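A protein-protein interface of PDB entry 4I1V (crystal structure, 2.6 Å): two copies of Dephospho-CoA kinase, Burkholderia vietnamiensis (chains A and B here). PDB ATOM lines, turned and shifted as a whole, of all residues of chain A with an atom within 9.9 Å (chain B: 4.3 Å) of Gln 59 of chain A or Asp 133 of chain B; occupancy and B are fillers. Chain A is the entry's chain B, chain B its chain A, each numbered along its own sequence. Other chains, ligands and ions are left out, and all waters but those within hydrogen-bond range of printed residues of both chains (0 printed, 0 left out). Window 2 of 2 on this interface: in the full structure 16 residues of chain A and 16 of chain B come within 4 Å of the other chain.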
ATOM      1  N   ALA A  53      15.930  -7.919   9.794  1.00  0.00           N
ATOM      2  CA  ALA A  53      16.977  -8.906   9.502  1.00  0.00           C
ATOM      3  C   ALA A  53      16.468 -10.325   9.328  1.00  0.00           C
ATOM      4  O   ALA A  53      17.211 -11.207   8.885  1.00  0.00           O
ATOM      5  CB  ALA A  53      18.017  -8.898  10.609  1.00  0.00           C
ATOM      6  N   MET A  54      15.218 -10.568   9.678  1.00  0.00           N
ATOM      7  CA  MET A  54      14.715 -11.958   9.708  1.00  0.00           C
ATOM      8  C   MET A  54      14.584 -12.645   8.354  1.00  0.00           C
ATOM      9  O   MET A  54      14.910 -13.833   8.235  1.00  0.00           O
ATOM     10  CB  MET A  54      13.400 -12.030  10.490  1.00  0.00           C
ATOM     11  CG  MET A  54      13.560 -11.660  11.963  1.00  0.00           C
ATOM     12  SD  MET A  54      14.859 -12.591  12.793  1.00  0.00           S
ATOM     13  CE  MET A  54      14.300 -14.266  12.506  1.00  0.00           C
ATOM     14  N   PRO A  55      14.107 -11.930   7.329  1.00  0.00           N
ATOM     15  CA  PRO A  55      14.048 -12.598   6.010  1.00  0.00           C
ATOM     16  C   PRO A  55      15.416 -13.155   5.629  1.00  0.00           C
ATOM     17  O   PRO A  55      15.550 -14.332   5.299  1.00  0.00           O
ATOM     18  CB  PRO A  55      13.626 -11.474   5.066  1.00  0.00           C
ATOM     19  CG  PRO A  55      12.823 -10.559   5.937  1.00  0.00           C
ATOM     20  CD  PRO A  55      13.509 -10.585   7.288  1.00  0.00           C
ATOM     21  N   ALA A  56      16.436 -12.322   5.750  1.00  0.00           N
ATOM     22  CA  ALA A  56      17.776 -12.746   5.393  1.00  0.00           C
ATOM     23  C   ALA A  56      18.231 -13.928   6.258  1.00  0.00           C
ATOM     24  O   ALA A  56      18.926 -14.825   5.763  1.00  0.00           O
ATOM     25  CB  ALA A  56      18.738 -11.573   5.481  1.00  0.00           C
ATOM     26  N   ILE A  57      17.826 -13.942   7.529  1.00  0.00           N
ATOM     27  CA  ILE A  57      18.296 -14.980   8.458  1.00  0.00           C
ATOM     28  C   ILE A  57      17.614 -16.315   8.209  1.00  0.00           C
ATOM     29  O   ILE A  57      18.251 -17.359   8.266  1.00  0.00           O
ATOM     30  CB  ILE A  57      18.099 -14.591   9.927  1.00  0.00           C
ATOM     31  CG1 ILE A  57      19.074 -13.497  10.326  1.00  0.00           C
ATOM     32  CG2 ILE A  57      18.363 -15.778  10.829  1.00  0.00           C
ATOM     33  CD1 ILE A  57      18.732 -12.778  11.607  1.00  0.00           C
ATOM     34  N   GLU A  58      16.321 -16.280   7.932  1.00  0.00           N
ATOM     35  CA  GLU A  58      15.631 -17.472   7.531  1.00  0.00           C
ATOM     36  C   GLU A  58      16.242 -18.022   6.226  1.00  0.00           C
ATOM     37  O   GLU A  58      16.599 -19.204   6.122  1.00  0.00           O
ATOM     38  CB  GLU A  58      14.147 -17.165   7.367  1.00  0.00           C
ATOM     39  CG  GLU A  58      13.328 -18.331   6.830  1.00  0.00           C
ATOM     40  CD  GLU A  58      11.846 -18.076   6.945  1.00  0.00           C
ATOM     41  OE1 GLU A  58      11.371 -17.835   8.067  1.00  0.00           O
ATOM     42  OE2 GLU A  58      11.150 -18.117   5.925  1.00  0.00           O
ATOM     43  N   GLN A  59      16.357 -17.161   5.231  1.00  0.00           N
ATOM     44  CA  GLN A  59      16.964 -17.557   3.979  1.00  0.00           C
ATOM     45  C   GLN A  59      18.336 -18.208   4.196  1.00  0.00           C
ATOM     46  O   GLN A  59      18.597 -19.296   3.703  1.00  0.00           O
ATOM     47  CB  GLN A  59      17.074 -16.360   3.038  1.00  0.00           C
ATOM     48  CG  GLN A  59      17.842 -16.670   1.752  1.00  0.00           C
ATOM     49  CD  GLN A  59      17.232 -17.785   0.922  1.00  0.00           C
ATOM     50  OE1 GLN A  59      17.955 -18.585   0.328  1.00  0.00           O
ATOM     51  NE2 GLN A  59      15.903 -17.842   0.872  1.00  0.00           N
ATOM     52  N   THR A  60      19.200 -17.544   4.934  1.00  0.00           N
ATOM     53  CA  THR A  60      20.582 -18.005   5.068  1.00  0.00           C
ATOM     54  C   THR A  60      20.763 -19.180   6.033  1.00  0.00           C
ATOM     55  O   THR A  60      21.661 -19.990   5.842  1.00  0.00           O
ATOM     56  CB  THR A  60      21.510 -16.843   5.485  1.00  0.00           C
ATOM     57  OG1 THR A  60      21.665 -15.936   4.374  1.00  0.00           O
ATOM     58  CG2 THR A  60      22.884 -17.355   5.910  1.00  0.00           C
ATOM     59  N   PHE A  61      19.924 -19.282   7.050  1.00  0.00           N
ATOM     60  CA  PHE A  61      20.098 -20.306   8.079  1.00  0.00           C
ATOM     61  C   PHE A  61      18.994 -21.349   8.112  1.00  0.00           C
ATOM     62  O   PHE A  61      19.216 -22.427   8.654  1.00  0.00           O
ATOM     63  CB  PHE A  61      20.192 -19.661   9.457  1.00  0.00           C
ATOM     64  CG  PHE A  61      21.495 -18.988   9.715  1.00  0.00           C
ATOM     65  CD1 PHE A  61      21.634 -17.621   9.528  1.00  0.00           C
ATOM     66  CD2 PHE A  61      22.599 -19.724  10.119  1.00  0.00           C
ATOM     67  CE1 PHE A  61      22.852 -16.999   9.746  1.00  0.00           C
ATOM     68  CE2 PHE A  61      23.818 -19.111  10.335  1.00  0.00           C
ATOM     69  CZ  PHE A  61      23.945 -17.746  10.153  1.00  0.00           C
ATOM     70  N   GLY A  62      17.815 -21.023   7.570  1.00  0.00           N
ATOM     71  CA  GLY A  62      16.648 -21.925   7.563  1.00  0.00           C
ATOM     72  C   GLY A  62      15.665 -21.668   8.700  1.00  0.00           C
ATOM     73  O   GLY A  62      16.041 -21.100   9.716  1.00  0.00           O
ATOM     74  N   PRO A  63      14.392 -22.094   8.534  1.00  0.00           N
ATOM     75  CA  PRO A  63      13.325 -21.983   9.556  1.00  0.00           C
ATOM     76  C   PRO A  63      13.633 -22.650  10.894  1.00  0.00           C
ATOM     77  O   PRO A  63      12.943 -22.398  11.889  1.00  0.00           O
ATOM     78  CB  PRO A  63      12.138 -22.685   8.903  1.00  0.00           C
ATOM     79  CG  PRO A  63      12.360 -22.504   7.445  1.00  0.00           C
ATOM     80  CD  PRO A  63      13.848 -22.560   7.240  1.00  0.00           C
ATOM     81  N   ALA A  64      14.641 -23.511  10.911  1.00  0.00           N
ATOM     82  CA  ALA A  64      15.165 -24.047  12.158  1.00  0.00           C
ATOM     83  C   ALA A  64      15.461 -22.959  13.187  1.00  0.00           C
ATOM     84  O   ALA A  64      15.228 -23.170  14.371  1.00  0.00           O
ATOM     85  CB  ALA A  64      16.422 -24.858  11.883  1.00  0.00           C
ATOM     86  N   PHE A  65      15.971 -21.808  12.731  1.00  0.00           N
ATOM     87  CA  PHE A  65      16.426 -20.727  13.614  1.00  0.00           C
ATOM     88  C   PHE A  65      15.441 -19.567  13.754  1.00  0.00           C
ATOM     89  O   PHE A  65      15.770 -18.508  14.304  1.00  0.00           O
ATOM     90  CB  PHE A  65      17.738 -20.183  13.105  1.00  0.00           C
ATOM     91  CG  PHE A  65      18.804 -21.209  13.016  1.00  0.00           C
ATOM     92  CD1 PHE A  65      19.708 -21.376  14.065  1.00  0.00           C
ATOM     93  CD2 PHE A  65      18.905 -22.033  11.894  1.00  0.00           C
ATOM     94  CE1 PHE A  65      20.703 -22.339  13.992  1.00  0.00           C
ATOM     95  CE2 PHE A  65      19.890 -23.006  11.815  1.00  0.00           C
ATOM     96  CZ  PHE A  65      20.790 -23.160  12.866  1.00  0.00           C
ATOM     97  N   VAL A  66      14.238 -19.768  13.248  1.00  0.00           N
ATOM     98  CA  VAL A  66      13.161 -18.813  13.407  1.00  0.00           C
ATOM     99  C   VAL A  66      12.225 -19.479  14.349  1.00  0.00           C
ATOM    100  O   VAL A  66      11.751 -20.585  14.067  1.00  0.00           O
ATOM    101  CB  VAL A  66      12.441 -18.531  12.063  1.00  0.00           C
ATOM    102  CG1 VAL A  66      11.203 -17.661  12.273  1.00  0.00           C
ATOM    103  CG2 VAL A  66      13.415 -17.888  11.075  1.00  0.00           C
ATOM    104  N   MET A  77      20.806 -20.198  17.907  1.00  0.00           N
ATOM    105  CA  MET A  77      21.816 -19.380  17.249  1.00  0.00           C
ATOM    106  C   MET A  77      22.980 -19.145  18.197  1.00  0.00           C
ATOM    107  O   MET A  77      24.131 -19.336  17.805  1.00  0.00           O
ATOM    108  CB  MET A  77      21.219 -18.035  16.802  1.00  0.00           C
ATOM    109  CG  MET A  77      22.164 -17.119  16.028  1.00  0.00           C
ATOM    110  SD  MET A  77      22.691 -17.782  14.436  1.00  0.00           S
ATOM    111  CE  MET A  77      21.208 -17.524  13.464  1.00  0.00           C
ATOM    112  N   ARG A  90      28.774 -15.337   9.015  1.00  0.00           N
ATOM    113  CA  ARG A  90      27.597 -15.357   8.129  1.00  0.00           C
ATOM    114  C   ARG A  90      26.428 -14.561   8.713  1.00  0.00           C
ATOM    115  O   ARG A  90      25.764 -13.831   7.985  1.00  0.00           O
ATOM    116  CB  ARG A  90      27.170 -16.776   7.731  1.00  0.00           C
ATOM    117  CG  ARG A  90      27.492 -17.108   6.266  1.00  0.00           C
ATOM    118  CD  ARG A  90      26.988 -18.485   5.820  1.00  0.00           C
ATOM    119  NE  ARG A  90      27.412 -19.520   6.763  1.00  0.00           N
ATOM    120  CZ  ARG A  90      26.613 -20.228   7.564  1.00  0.00           C
ATOM    121  NH1 ARG A  90      27.146 -21.126   8.389  1.00  0.00           N
ATOM    122  NH2 ARG A  90      25.288 -20.073   7.543  1.00  0.00           N
ATOM    123  N   ILE A  94      24.946 -10.297   7.900  1.00  0.00           N
ATOM    124  CA  ILE A  94      23.585  -9.821   7.723  1.00  0.00           C
ATOM    125  C   ILE A  94      23.276  -8.678   8.672  1.00  0.00           C
ATOM    126  O   ILE A  94      22.723  -7.662   8.263  1.00  0.00           O
ATOM    127  CB  ILE A  94      22.567 -10.937   7.950  1.00  0.00           C
ATOM    128  CG1 ILE A  94      22.635 -11.939   6.787  1.00  0.00           C
ATOM    129  CG2 ILE A  94      21.156 -10.368   8.084  1.00  0.00           C
ATOM    130  CD1 ILE A  94      21.996 -13.265   7.119  1.00  0.00           C
ATOM    131  N   MET B   9       9.148 -14.684   1.992  1.00  0.00           N
ATOM    132  CA  MET B   9       9.260 -13.978   0.696  1.00  0.00           C
ATOM    133  C   MET B   9      10.232 -14.747  -0.205  1.00  0.00           C
ATOM    134  O   MET B   9      11.301 -15.146   0.252  1.00  0.00           O
ATOM    135  CB  MET B   9       9.720 -12.531   0.830  1.00  0.00           C
ATOM    136  N   TYR B  10       9.836 -15.005  -1.452  1.00  0.00           N
ATOM    137  CA  TYR B  10      10.708 -15.658  -2.420  1.00  0.00           C
ATOM    138  C   TYR B  10      11.544 -14.614  -3.155  1.00  0.00           C
ATOM    139  O   TYR B  10      10.998 -13.637  -3.677  1.00  0.00           O
ATOM    140  CB  TYR B  10       9.893 -16.473  -3.435  1.00  0.00           C
ATOM    141  CG  TYR B  10      10.713 -17.525  -4.157  1.00  0.00           C
ATOM    142  CD1 TYR B  10      11.115 -17.357  -5.474  1.00  0.00           C
ATOM    143  CD2 TYR B  10      11.111 -18.677  -3.501  1.00  0.00           C
ATOM    144  CE1 TYR B  10      11.880 -18.314  -6.104  1.00  0.00           C
ATOM    145  CE2 TYR B  10      11.860 -19.643  -4.131  1.00  0.00           C
ATOM    146  CZ  TYR B  10      12.250 -19.452  -5.427  1.00  0.00           C
ATOM    147  OH  TYR B  10      13.017 -20.429  -6.029  1.00  0.00           O
ATOM    148  N   ALA B  11      12.857 -14.852  -3.231  1.00  0.00           N
ATOM    149  CA  ALA B  11      13.778 -13.874  -3.827  1.00  0.00           C
ATOM    150  C   ALA B  11      14.648 -14.434  -4.940  1.00  0.00           C
ATOM    151  O   ALA B  11      15.290 -15.486  -4.791  1.00  0.00           O
ATOM    152  CB  ALA B  11      14.666 -13.278  -2.758  1.00  0.00           C
ATOM    153  N   ALA B 130      23.874 -16.424  -1.148  1.00  0.00           N
ATOM    154  CA  ALA B 130      23.156 -17.024  -0.009  1.00  0.00           C
ATOM    155  C   ALA B 130      21.825 -16.336   0.294  1.00  0.00           C
ATOM    156  O   ALA B 130      20.917 -16.950   0.853  1.00  0.00           O
ATOM    157  CB  ALA B 130      24.034 -16.970   1.225  1.00  0.00           C
ATOM    158  N   ARG B 131      21.729 -15.051  -0.029  1.00  0.00           N
ATOM    159  CA  ARG B 131      20.532 -14.265   0.257  1.00  0.00           C
ATOM    160  C   ARG B 131      19.359 -14.601  -0.685  1.00  0.00           C
ATOM    161  O   ARG B 131      18.199 -14.341  -0.363  1.00  0.00           O
ATOM    162  CB  ARG B 131      20.872 -12.774   0.159  1.00  0.00           C
ATOM    163  CG  ARG B 131      19.689 -11.822   0.351  1.00  0.00           C
ATOM    164  CD  ARG B 131      19.006 -12.052   1.685  1.00  0.00           C
ATOM    165  NE  ARG B 131      17.912 -11.106   1.898  1.00  0.00           N
ATOM    166  CZ  ARG B 131      16.644 -11.334   1.577  1.00  0.00           C
ATOM    167  NH1 ARG B 131      16.292 -12.449   0.974  1.00  0.00           N
ATOM    168  NH2 ARG B 131      15.722 -10.425   1.839  1.00  0.00           N
ATOM    169  N   CYS B 132      19.667 -15.160  -1.849  1.00  0.00           N
ATOM    170  CA  CYS B 132      18.668 -15.391  -2.859  1.00  0.00           C
ATOM    171  C   CYS B 132      18.261 -16.853  -2.892  1.00  0.00           C
ATOM    172  O   CYS B 132      19.110 -17.738  -2.731  1.00  0.00           O
ATOM    173  CB  CYS B 132      19.232 -15.016  -4.222  1.00  0.00           C
ATOM    174  SG  CYS B 132      19.665 -13.296  -4.450  1.00  0.00           S
ATOM    175  N   ASP B 133      16.975 -17.109  -3.144  1.00  0.00           N
ATOM    176  CA  ASP B 133      16.519 -18.464  -3.387  1.00  0.00           C
ATOM    177  C   ASP B 133      17.113 -19.000  -4.663  1.00  0.00           C
ATOM    178  O   ASP B 133      17.466 -20.169  -4.720  1.00  0.00           O
ATOM    179  CB  ASP B 133      14.994 -18.540  -3.478  1.00  0.00           C
ATOM    180  CG  ASP B 133      14.300 -18.156  -2.176  1.00  0.00           C
ATOM    181  OD1 ASP B 133      14.137 -19.053  -1.297  1.00  0.00           O
ATOM    182  OD2 ASP B 133      13.916 -16.964  -2.058  1.00  0.00           O
ATOM    183  N   ARG B 134      17.189 -18.160  -5.698  1.00  0.00           N
ATOM    184  CA  ARG B 134      17.723 -18.547  -7.002  1.00  0.00           C
ATOM    185  C   ARG B 134      18.523 -17.404  -7.621  1.00  0.00           C
ATOM    186  O   ARG B 134      18.247 -16.210  -7.387  1.00  0.00           O
ATOM    187  CB  ARG B 134      16.593 -18.851  -7.983  1.00  0.00           C
ATOM    188  CG  ARG B 134      15.795 -20.093  -7.678  1.00  0.00           C
ATOM    189  CD  ARG B 134      14.749 -20.387  -8.761  1.00  0.00           C
ATOM    190  NE  ARG B 134      15.280 -21.096  -9.938  1.00  0.00           N
ATOM    191  CZ  ARG B 134      15.646 -22.370  -9.945  1.00  0.00           C
ATOM    192  NH1 ARG B 134      15.541 -23.093  -8.855  1.00  0.00           N
ATOM    193  NH2 ARG B 134      16.118 -22.932 -11.048  1.00  0.00           N
ATOM    194  N   LYS B 209       6.740 -22.455  -0.923  1.00  0.00           N
ATOM    195  CA  LYS B 209       7.562 -22.047   0.187  1.00  0.00           C
ATOM    196  C   LYS B 209       6.646 -21.484   1.288  1.00  0.00           C
ATOM    197  O   LYS B 209       7.114 -21.176   2.394  1.00  0.00           O
ATOM    198  CB  LYS B 209       8.542 -20.994  -0.332  1.00  0.00           C
ATOM    199  CG  LYS B 209       9.928 -21.001   0.286  1.00  0.00           C
ATOM    200  CD  LYS B 209      10.390 -19.549   0.397  1.00  0.00           C
ATOM    201  CE  LYS B 209      11.781 -19.363   0.992  1.00  0.00           C
ATOM    202  NZ  LYS B 209      12.200 -17.967   0.767  1.00  0.00           N
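No position is printed for both chains. Of the 8 pairs that touch across the chains among the printed residues, none has its exchanged pair printed and touching as well.
The side-chain amide oxygen (OE1) of Gln 59 of chain A lies close to the backbone carbonyl oxygen (O) of Ala 130 of chain B (3.4 Å). OE1 of Gln 59 of chain A lies close to O of Cys 132 of chain B, 3.4 Å away. The side-chain carboxylate (OD1) of Asp 133 of chain B sits at hydrogen-bond distance from the side-chain amide nitrogen (NE2) of Gln 59 of chain A (3.0 Å).
Of the 17 printed residues of chain A, 4 touch a printed residue of chain B. Among the printed residues, 8 pairs touch across the chains. Among the printed residues, no Asp or Glu carboxylate lies within 4 Å of a Lys or Arg side-chain nitrogen of the other chain.
Of chain A, only Gln 59 comes within 4 Å of Asp 133 of chain B. No residue of chain A comes within 4 Å of Ala 11 of chain B. Of the printed residues of chain A, Arg 131 of chain B touches Pro 55, Ala 56 and Gln 59. Of the printed residues of chain B, Pro 55 of chain A touches Arg 131 (3.99 Å). Printed residues of chain B within 4 Å of Ala 56 of chain A: Arg 131 (3.7 Å). Met 9 of chain B touches none of the printed residues of chain A. Ile 57 of chain A touches none of the printed residues of chain B. The nearest printed residue of chain A that does not touch Arg 131 of chain B is Thr 60 of chain A (4.5 Å).
Among the printed residues, pairs that only touch across the chains: Gln 59 of chain A with Arg 131 of chain B (3.2 Å), Ala 56 of chain A with Arg 131 of chain B (3.7 Å), Gln 59 of chain A with Lys 209 of chain B (3.7 Å), Thr 60 of chain A with Ala 130 of chain B (3.7 Å) and Pro 55 of chain A with Arg 131 of chain B (3.99 Å).
O of Met 9 of chain B lies within hydrogen-bond range of NZ of Lys 209 of chain B (3.0 Å). The backbone NH (N) of Ala 11 of chain B sits at hydrogen-bond distance from the side-chain carboxylate (OD2) of Asp 133 of chain B, 2.6 Å away. OD1 of Asp 133 of chain B lies within salt-bridge range of NZ of Lys 209 of chain B (3.0 Å). The backbone carbonyl oxygen (O) of Ala 56 of chain A sits at hydrogen-bond distance from the side-chain hydroxyl (OG1) of Thr 60 of chain A, at 3.3 Å.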
